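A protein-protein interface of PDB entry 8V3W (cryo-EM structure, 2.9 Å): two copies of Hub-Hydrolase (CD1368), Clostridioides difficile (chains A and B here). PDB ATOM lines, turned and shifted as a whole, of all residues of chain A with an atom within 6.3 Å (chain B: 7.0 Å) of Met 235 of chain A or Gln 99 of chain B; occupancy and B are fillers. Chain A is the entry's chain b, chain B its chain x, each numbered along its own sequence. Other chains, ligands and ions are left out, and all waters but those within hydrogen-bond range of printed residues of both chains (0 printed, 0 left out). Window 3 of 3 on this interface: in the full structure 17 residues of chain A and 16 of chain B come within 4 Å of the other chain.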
ATOM      1  N   MET A 202     -15.169   8.432  -1.654  1.00  0.00           N
ATOM      2  CA  MET A 202     -16.359   7.974  -2.353  1.00  0.00           C
ATOM      3  C   MET A 202     -17.601   8.756  -1.932  1.00  0.00           C
ATOM      4  O   MET A 202     -18.679   8.548  -2.496  1.00  0.00           O
ATOM      5  CB  MET A 202     -16.519   6.463  -2.105  1.00  0.00           C
ATOM      6  CG  MET A 202     -17.861   5.819  -2.358  1.00  0.00           C
ATOM      7  SD  MET A 202     -17.884   4.092  -1.864  1.00  0.00           S
ATOM      8  CE  MET A 202     -19.585   3.927  -1.356  1.00  0.00           C
ATOM      9  N   GLU A 203     -17.455   9.713  -1.013  1.00  0.00           N
ATOM     10  CA  GLU A 203     -18.609  10.332  -0.368  1.00  0.00           C
ATOM     11  C   GLU A 203     -19.499  11.077  -1.358  1.00  0.00           C
ATOM     12  O   GLU A 203     -20.730  11.015  -1.256  1.00  0.00           O
ATOM     13  CB  GLU A 203     -18.135  11.273   0.735  1.00  0.00           C
ATOM     14  CG  GLU A 203     -17.584  10.558   1.950  1.00  0.00           C
ATOM     15  CD  GLU A 203     -16.684  11.439   2.785  1.00  0.00           C
ATOM     16  OE1 GLU A 203     -16.422  12.584   2.366  1.00  0.00           O
ATOM     17  OE2 GLU A 203     -16.230  10.987   3.855  1.00  0.00           O
ATOM     18  N   VAL A 205     -20.096  10.732  -4.647  1.00  0.00           N
ATOM     19  CA  VAL A 205     -20.306  10.022  -5.903  1.00  0.00           C
ATOM     20  C   VAL A 205     -21.778  10.089  -6.283  1.00  0.00           C
ATOM     21  O   VAL A 205     -22.659   9.979  -5.427  1.00  0.00           O
ATOM     22  CB  VAL A 205     -19.823   8.564  -5.784  1.00  0.00           C
ATOM     23  CG1 VAL A 205     -20.415   7.699  -6.877  1.00  0.00           C
ATOM     24  CG2 VAL A 205     -18.315   8.508  -5.834  1.00  0.00           C
ATOM     25  N   LYS A 206     -22.047  10.287  -7.573  1.00  0.00           N
ATOM     26  CA  LYS A 206     -23.396  10.227  -8.123  1.00  0.00           C
ATOM     27  C   LYS A 206     -23.366   9.420  -9.411  1.00  0.00           C
ATOM     28  O   LYS A 206     -22.558   9.704 -10.299  1.00  0.00           O
ATOM     29  CB  LYS A 206     -23.947  11.629  -8.391  1.00  0.00           C
ATOM     30  CG  LYS A 206     -25.207  11.949  -7.625  1.00  0.00           C
ATOM     31  CD  LYS A 206     -24.897  12.503  -6.253  1.00  0.00           C
ATOM     32  CE  LYS A 206     -26.028  12.211  -5.289  1.00  0.00           C
ATOM     33  NZ  LYS A 206     -25.765  12.743  -3.929  1.00  0.00           N
ATOM     34  N   ASN A 207     -24.245   8.419  -9.522  1.00  0.00           N
ATOM     35  CA  ASN A 207     -24.281   7.579 -10.714  1.00  0.00           C
ATOM     36  C   ASN A 207     -25.691   7.324 -11.235  1.00  0.00           C
ATOM     37  O   ASN A 207     -25.870   6.440 -12.078  1.00  0.00           O
ATOM     38  CB  ASN A 207     -23.566   6.242 -10.468  1.00  0.00           C
ATOM     39  CG  ASN A 207     -24.114   5.484  -9.276  1.00  0.00           C
ATOM     40  OD1 ASN A 207     -25.302   5.537  -8.979  1.00  0.00           O
ATOM     41  ND2 ASN A 207     -23.244   4.749  -8.601  1.00  0.00           N
ATOM     42  N   LYS A 208     -26.691   8.058 -10.760  1.00  0.00           N
ATOM     43  CA  LYS A 208     -28.040   7.980 -11.302  1.00  0.00           C
ATOM     44  C   LYS A 208     -28.639   9.376 -11.332  1.00  0.00           C
ATOM     45  O   LYS A 208     -28.498  10.135 -10.371  1.00  0.00           O
ATOM     46  CB  LYS A 208     -28.934   7.049 -10.480  1.00  0.00           C
ATOM     47  CG  LYS A 208     -30.151   6.548 -11.230  1.00  0.00           C
ATOM     48  CD  LYS A 208     -31.130   5.879 -10.288  1.00  0.00           C
ATOM     49  CE  LYS A 208     -31.978   4.846 -11.001  1.00  0.00           C
ATOM     50  NZ  LYS A 208     -33.132   5.454 -11.706  1.00  0.00           N
ATOM     51  N   VAL A 209     -29.309   9.706 -12.432  1.00  0.00           N
ATOM     52  CA  VAL A 209     -29.903  11.023 -12.626  1.00  0.00           C
ATOM     53  C   VAL A 209     -31.374  10.848 -12.962  1.00  0.00           C
ATOM     54  O   VAL A 209     -31.719  10.091 -13.875  1.00  0.00           O
ATOM     55  CB  VAL A 209     -29.192  11.815 -13.739  1.00  0.00           C
ATOM     56  CG1 VAL A 209     -29.838  13.177 -13.909  1.00  0.00           C
ATOM     57  CG2 VAL A 209     -27.717  11.961 -13.427  1.00  0.00           C
ATOM     58  N   VAL A 231     -18.433   1.327  -8.035  1.00  0.00           N
ATOM     59  CA  VAL A 231     -19.228   1.229  -6.814  1.00  0.00           C
ATOM     60  C   VAL A 231     -20.488   0.435  -7.135  1.00  0.00           C
ATOM     61  O   VAL A 231     -21.257   0.810  -8.026  1.00  0.00           O
ATOM     62  CB  VAL A 231     -19.563   2.614  -6.233  1.00  0.00           C
ATOM     63  CG1 VAL A 231     -18.302   3.299  -5.757  1.00  0.00           C
ATOM     64  CG2 VAL A 231     -20.256   3.490  -7.253  1.00  0.00           C
ATOM     65  N   VAL A 233     -23.124   0.271  -5.645  1.00  0.00           N
ATOM     66  CA  VAL A 233     -24.334   0.907  -5.149  1.00  0.00           C
ATOM     67  C   VAL A 233     -24.826   1.972  -6.119  1.00  0.00           C
ATOM     68  O   VAL A 233     -24.071   2.501  -6.939  1.00  0.00           O
ATOM     69  CB  VAL A 233     -24.071   1.493  -3.755  1.00  0.00           C
ATOM     70  CG1 VAL A 233     -25.361   1.678  -3.047  1.00  0.00           C
ATOM     71  CG2 VAL A 233     -23.192   0.554  -2.976  1.00  0.00           C
ATOM     72  N   ILE A 234     -26.114   2.283  -6.018  1.00  0.00           N
ATOM     73  CA  ILE A 234     -26.748   3.347  -6.782  1.00  0.00           C
ATOM     74  C   ILE A 234     -26.971   4.529  -5.851  1.00  0.00           C
ATOM     75  O   ILE A 234     -27.658   4.402  -4.830  1.00  0.00           O
ATOM     76  CB  ILE A 234     -28.074   2.875  -7.396  1.00  0.00           C
ATOM     77  CG1 ILE A 234     -27.815   1.890  -8.533  1.00  0.00           C
ATOM     78  CG2 ILE A 234     -28.913   4.057  -7.844  1.00  0.00           C
ATOM     79  CD1 ILE A 234     -27.780   2.525  -9.897  1.00  0.00           C
ATOM     80  N   MET A 235     -26.396   5.676  -6.198  1.00  0.00           N
ATOM     81  CA  MET A 235     -26.613   6.926  -5.476  1.00  0.00           C
ATOM     82  C   MET A 235     -27.253   7.906  -6.447  1.00  0.00           C
ATOM     83  O   MET A 235     -26.609   8.348  -7.401  1.00  0.00           O
ATOM     84  CB  MET A 235     -25.309   7.482  -4.909  1.00  0.00           C
ATOM     85  CG  MET A 235     -24.392   6.445  -4.295  1.00  0.00           C
ATOM     86  SD  MET A 235     -23.555   7.073  -2.827  1.00  0.00           S
ATOM     87  CE  MET A 235     -22.021   6.165  -2.895  1.00  0.00           C
ATOM     88  N   GLN A 236     -28.511   8.249  -6.199  1.00  0.00           N
ATOM     89  CA  GLN A 236     -29.317   8.966  -7.172  1.00  0.00           C
ATOM     90  C   GLN A 236     -29.261  10.473  -6.951  1.00  0.00           C
ATOM     91  O   GLN A 236     -28.948  10.963  -5.866  1.00  0.00           O
ATOM     92  CB  GLN A 236     -30.767   8.489  -7.117  1.00  0.00           C
ATOM     93  CG  GLN A 236     -31.546   9.039  -5.949  1.00  0.00           C
ATOM     94  CD  GLN A 236     -33.031   8.788  -6.063  1.00  0.00           C
ATOM     95  OE1 GLN A 236     -33.463   7.806  -6.665  1.00  0.00           O
ATOM     96  NE2 GLN A 236     -33.825   9.677  -5.481  1.00  0.00           N
ATOM     97  N   LYS A 237     -29.576  11.203  -8.016  1.00  0.00           N
ATOM     98  CA  LYS A 237     -29.664  12.654  -8.011  1.00  0.00           C
ATOM     99  C   LYS A 237     -30.931  13.061  -8.746  1.00  0.00           C
ATOM    100  O   LYS A 237     -31.325  12.412  -9.718  1.00  0.00           O
ATOM    101  CB  LYS A 237     -28.444  13.281  -8.684  1.00  0.00           C
ATOM    102  CG  LYS A 237     -28.382  14.787  -8.599  1.00  0.00           C
ATOM    103  CD  LYS A 237     -27.125  15.301  -9.263  1.00  0.00           C
ATOM    104  CE  LYS A 237     -26.732  16.660  -8.723  1.00  0.00           C
ATOM    105  NZ  LYS A 237     -25.283  16.917  -8.933  1.00  0.00           N
ATOM    106  N   MET B  73     -18.694  -1.576   3.388  1.00  0.00           N
ATOM    107  CA  MET B  73     -17.983  -1.080   2.221  1.00  0.00           C
ATOM    108  C   MET B  73     -16.884  -0.110   2.631  1.00  0.00           C
ATOM    109  O   MET B  73     -17.014   0.616   3.618  1.00  0.00           O
ATOM    110  CB  MET B  73     -18.954  -0.372   1.281  1.00  0.00           C
ATOM    111  CG  MET B  73     -18.465  -0.217  -0.135  1.00  0.00           C
ATOM    112  SD  MET B  73     -19.821   0.062  -1.283  1.00  0.00           S
ATOM    113  CE  MET B  73     -21.080   0.614  -0.147  1.00  0.00           C
ATOM    114  N   ILE B  75     -14.891   3.264   2.136  1.00  0.00           N
ATOM    115  CA  ILE B  75     -15.331   4.569   1.667  1.00  0.00           C
ATOM    116  C   ILE B  75     -14.170   5.540   1.488  1.00  0.00           C
ATOM    117  O   ILE B  75     -14.109   6.255   0.484  1.00  0.00           O
ATOM    118  CB  ILE B  75     -16.394   5.163   2.614  1.00  0.00           C
ATOM    119  CG1 ILE B  75     -17.615   4.248   2.644  1.00  0.00           C
ATOM    120  CG2 ILE B  75     -16.773   6.567   2.182  1.00  0.00           C
ATOM    121  CD1 ILE B  75     -18.866   4.921   3.063  1.00  0.00           C
ATOM    122  N   GLY B  94     -26.302   0.427   6.301  1.00  0.00           N
ATOM    123  CA  GLY B  94     -27.448   1.222   6.704  1.00  0.00           C
ATOM    124  C   GLY B  94     -27.551   2.579   6.043  1.00  0.00           C
ATOM    125  O   GLY B  94     -28.622   3.190   6.076  1.00  0.00           O
ATOM    126  N   PHE B  95     -26.474   3.068   5.433  1.00  0.00           N
ATOM    127  CA  PHE B  95     -26.546   4.376   4.795  1.00  0.00           C
ATOM    128  C   PHE B  95     -27.317   4.347   3.484  1.00  0.00           C
ATOM    129  O   PHE B  95     -27.503   5.403   2.875  1.00  0.00           O
ATOM    130  CB  PHE B  95     -25.136   4.947   4.586  1.00  0.00           C
ATOM    131  CG  PHE B  95     -24.395   4.371   3.414  1.00  0.00           C
ATOM    132  CD1 PHE B  95     -23.637   3.226   3.559  1.00  0.00           C
ATOM    133  CD2 PHE B  95     -24.417   4.996   2.182  1.00  0.00           C
ATOM    134  CE1 PHE B  95     -22.944   2.701   2.492  1.00  0.00           C
ATOM    135  CE2 PHE B  95     -23.725   4.474   1.113  1.00  0.00           C
ATOM    136  CZ  PHE B  95     -22.988   3.327   1.268  1.00  0.00           C
ATOM    137  N   LEU B  96     -27.769   3.174   3.039  1.00  0.00           N
ATOM    138  CA  LEU B  96     -28.545   3.086   1.810  1.00  0.00           C
ATOM    139  C   LEU B  96     -29.959   3.618   1.975  1.00  0.00           C
ATOM    140  O   LEU B  96     -30.606   3.941   0.974  1.00  0.00           O
ATOM    141  CB  LEU B  96     -28.612   1.641   1.331  1.00  0.00           C
ATOM    142  CG  LEU B  96     -27.242   1.091   0.965  1.00  0.00           C
ATOM    143  CD1 LEU B  96     -27.324  -0.325   0.420  1.00  0.00           C
ATOM    144  CD2 LEU B  96     -26.547   2.034   0.033  1.00  0.00           C
ATOM    145  N   LEU B  97     -30.461   3.689   3.208  1.00  0.00           N
ATOM    146  CA  LEU B  97     -31.810   4.192   3.432  1.00  0.00           C
ATOM    147  C   LEU B  97     -31.909   5.675   3.104  1.00  0.00           C
ATOM    148  O   LEU B  97     -32.889   6.116   2.493  1.00  0.00           O
ATOM    149  CB  LEU B  97     -32.226   3.944   4.880  1.00  0.00           C
ATOM    150  CG  LEU B  97     -32.977   2.661   5.224  1.00  0.00           C
ATOM    151  CD1 LEU B  97     -33.111   2.546   6.724  1.00  0.00           C
ATOM    152  CD2 LEU B  97     -34.342   2.627   4.566  1.00  0.00           C
ATOM    153  N   THR B  98     -30.908   6.460   3.501  1.00  0.00           N
ATOM    154  CA  THR B  98     -30.961   7.905   3.317  1.00  0.00           C
ATOM    155  C   THR B  98     -30.766   8.332   1.868  1.00  0.00           C
ATOM    156  O   THR B  98     -30.985   9.505   1.557  1.00  0.00           O
ATOM    157  CB  THR B  98     -29.910   8.586   4.196  1.00  0.00           C
ATOM    158  OG1 THR B  98     -28.628   8.500   3.568  1.00  0.00           O
ATOM    159  CG2 THR B  98     -29.837   7.912   5.551  1.00  0.00           C
ATOM    160  N   GLN B  99     -30.354   7.425   0.981  1.00  0.00           N
ATOM    161  CA  GLN B  99     -30.248   7.776  -0.431  1.00  0.00           C
ATOM    162  C   GLN B  99     -31.617   7.825  -1.096  1.00  0.00           C
ATOM    163  O   GLN B  99     -31.853   8.650  -1.985  1.00  0.00           O
ATOM    164  CB  GLN B  99     -29.337   6.788  -1.156  1.00  0.00           C
ATOM    165  CG  GLN B  99     -27.974   6.620  -0.518  1.00  0.00           C
ATOM    166  CD  GLN B  99     -27.133   7.876  -0.616  1.00  0.00           C
ATOM    167  OE1 GLN B  99     -27.034   8.488  -1.678  1.00  0.00           O
ATOM    168  NE2 GLN B  99     -26.524   8.268   0.493  1.00  0.00           N
ATOM    169  N   SER B 100     -32.526   6.949  -0.686  1.00  0.00           N
ATOM    170  CA  SER B 100     -33.859   6.912  -1.267  1.00  0.00           C
ATOM    171  C   SER B 100     -34.650   8.160  -0.895  1.00  0.00           C
ATOM    172  O   SER B 100     -34.463   8.747   0.172  1.00  0.00           O
ATOM    173  CB  SER B 100     -34.603   5.662  -0.802  1.00  0.00           C
ATOM    174  OG  SER B 100     -34.588   5.565   0.610  1.00  0.00           O
ATOM    175  N   GLU B 101     -35.545   8.564  -1.798  1.00  0.00           N
ATOM    176  CA  GLU B 101     -36.339   9.777  -1.606  1.00  0.00           C
ATOM    177  C   GLU B 101     -37.629   9.624  -2.408  1.00  0.00           C
ATOM    178  O   GLU B 101     -37.637   9.865  -3.618  1.00  0.00           O
ATOM    179  CB  GLU B 101     -35.551  11.004  -2.038  1.00  0.00           C
ATOM    180  CG  GLU B 101     -36.266  12.319  -1.839  1.00  0.00           C
ATOM    181  CD  GLU B 101     -35.577  13.199  -0.821  1.00  0.00           C
ATOM    182  OE1 GLU B 101     -34.475  12.834  -0.360  1.00  0.00           O
ATOM    183  OE2 GLU B 101     -36.124  14.268  -0.498  1.00  0.00           O
ATOM    184  N   VAL B 102     -38.711   9.238  -1.731  1.00  0.00           N
ATOM    185  CA  VAL B 102     -39.971   8.922  -2.390  1.00  0.00           C
ATOM    186  C   VAL B 102     -41.092   9.722  -1.739  1.00  0.00           C
ATOM    187  O   VAL B 102     -40.975  10.200  -0.609  1.00  0.00           O
ATOM    188  CB  VAL B 102     -40.288   7.408  -2.340  1.00  0.00           C
ATOM    189  CG1 VAL B 102     -41.335   7.031  -3.381  1.00  0.00           C
ATOM    190  CG2 VAL B 102     -39.025   6.584  -2.535  1.00  0.00           C
ATOM    191  N   ASN B 144     -36.706  11.245   3.151  1.00  0.00           N
ATOM    192  CA  ASN B 144     -35.958   9.997   3.148  1.00  0.00           C
ATOM    193  C   ASN B 144     -36.824   8.839   3.631  1.00  0.00           C
ATOM    194  O   ASN B 144     -37.862   9.023   4.268  1.00  0.00           O
ATOM    195  CB  ASN B 144     -34.733  10.105   4.053  1.00  0.00           C
ATOM    196  CG  ASN B 144     -33.571  10.772   3.378  1.00  0.00           C
ATOM    197  OD1 ASN B 144     -33.476  10.782   2.155  1.00  0.00           O
ATOM    198  ND2 ASN B 144     -32.675  11.340   4.172  1.00  0.00           N
ATOM    199  N   GLY B 145     -36.382   7.623   3.311  1.00  0.00           N
ATOM    200  CA  GLY B 145     -37.009   6.451   3.895  1.00  0.00           C
ATOM    201  C   GLY B 145     -36.737   6.341   5.381  1.00  0.00           C
ATOM    202  O   GLY B 145     -37.624   5.984   6.164  1.00  0.00           O
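Among the printed residues, pairs that only touch across the chains: Val 233 of chain A with Leu 96 of chain B, Val 233 of chain A with Met 73 of chain B, Met 235 of chain A with Gln 99 of chain B, Met 202 of chain A with Met 73 of chain B and Gln 236 of chain A with Gln 99 of chain B.
Of the 13 printed residues of chain A, 4 touch a printed residue of chain B. Hydrophobic or aromatic side chains of chain A within 4 Å of the printed part of chain B: Met 202, Val 233 and Met 235. Of the 13 printed residues of chain B, 4 touch a printed residue of chain A. Hydrophobic or aromatic side chains of chain B within 4 Å of the printed part of chain A: Met 73 and Leu 96. Among the printed residues, 6 pairs touch across the chains. Among the printed residues, no Asp or Glu carboxylate lies within 4 Å of a Lys or Arg side-chain nitrogen of the other chain.
The backbone carbonyl oxygen (O) of Ile 75 of chain B sits at hydrogen-bond distance from the backbone NH (N) of Met 202 of chain A (3.2 Å).
No position is printed for both chains.
The side-chain amide nitrogen of Asn 207 of chain A is in hydrogen-bond range of the backbone carbonyl oxygen of Val 233 of chain A, at 2.9 Å. The backbone NH of Lys 208 of chain A lies within hydrogen-bond range of the backbone carbonyl oxygen of Met 235 of chain A (3.4 Å). OD1 of Asn 207 of chain A sits at hydrogen-bond distance from N of Met 235 of chain A, at 3.0 Å.
Of chain B, only Gln 99 (3.8 Å) comes within 4 Å of Met 235 of chain A. Of the printed residues of chain A, Ile 75 of chain B touches Met 202. Of the printed residues of chain B, Met 202 of chain A touches Met 73 and Ile 75. Of the printed residues of chain A, Met 73 of chain B touches Met 202 (3.8 Å) and Val 233 (3.5 Å). Of the printed residues of chain B, Val 233 of chain A touches Met 73 (3.5 Å) and Leu 96 (3.3 Å). The nearest residue of chain B that does not touch Met 235 of chain A is Phe 95 of chain B (4.7 Å). The nearest printed residue of chain B that does not touch Val 233 of chain A is Phe 95 of chain B (5.1 Å).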
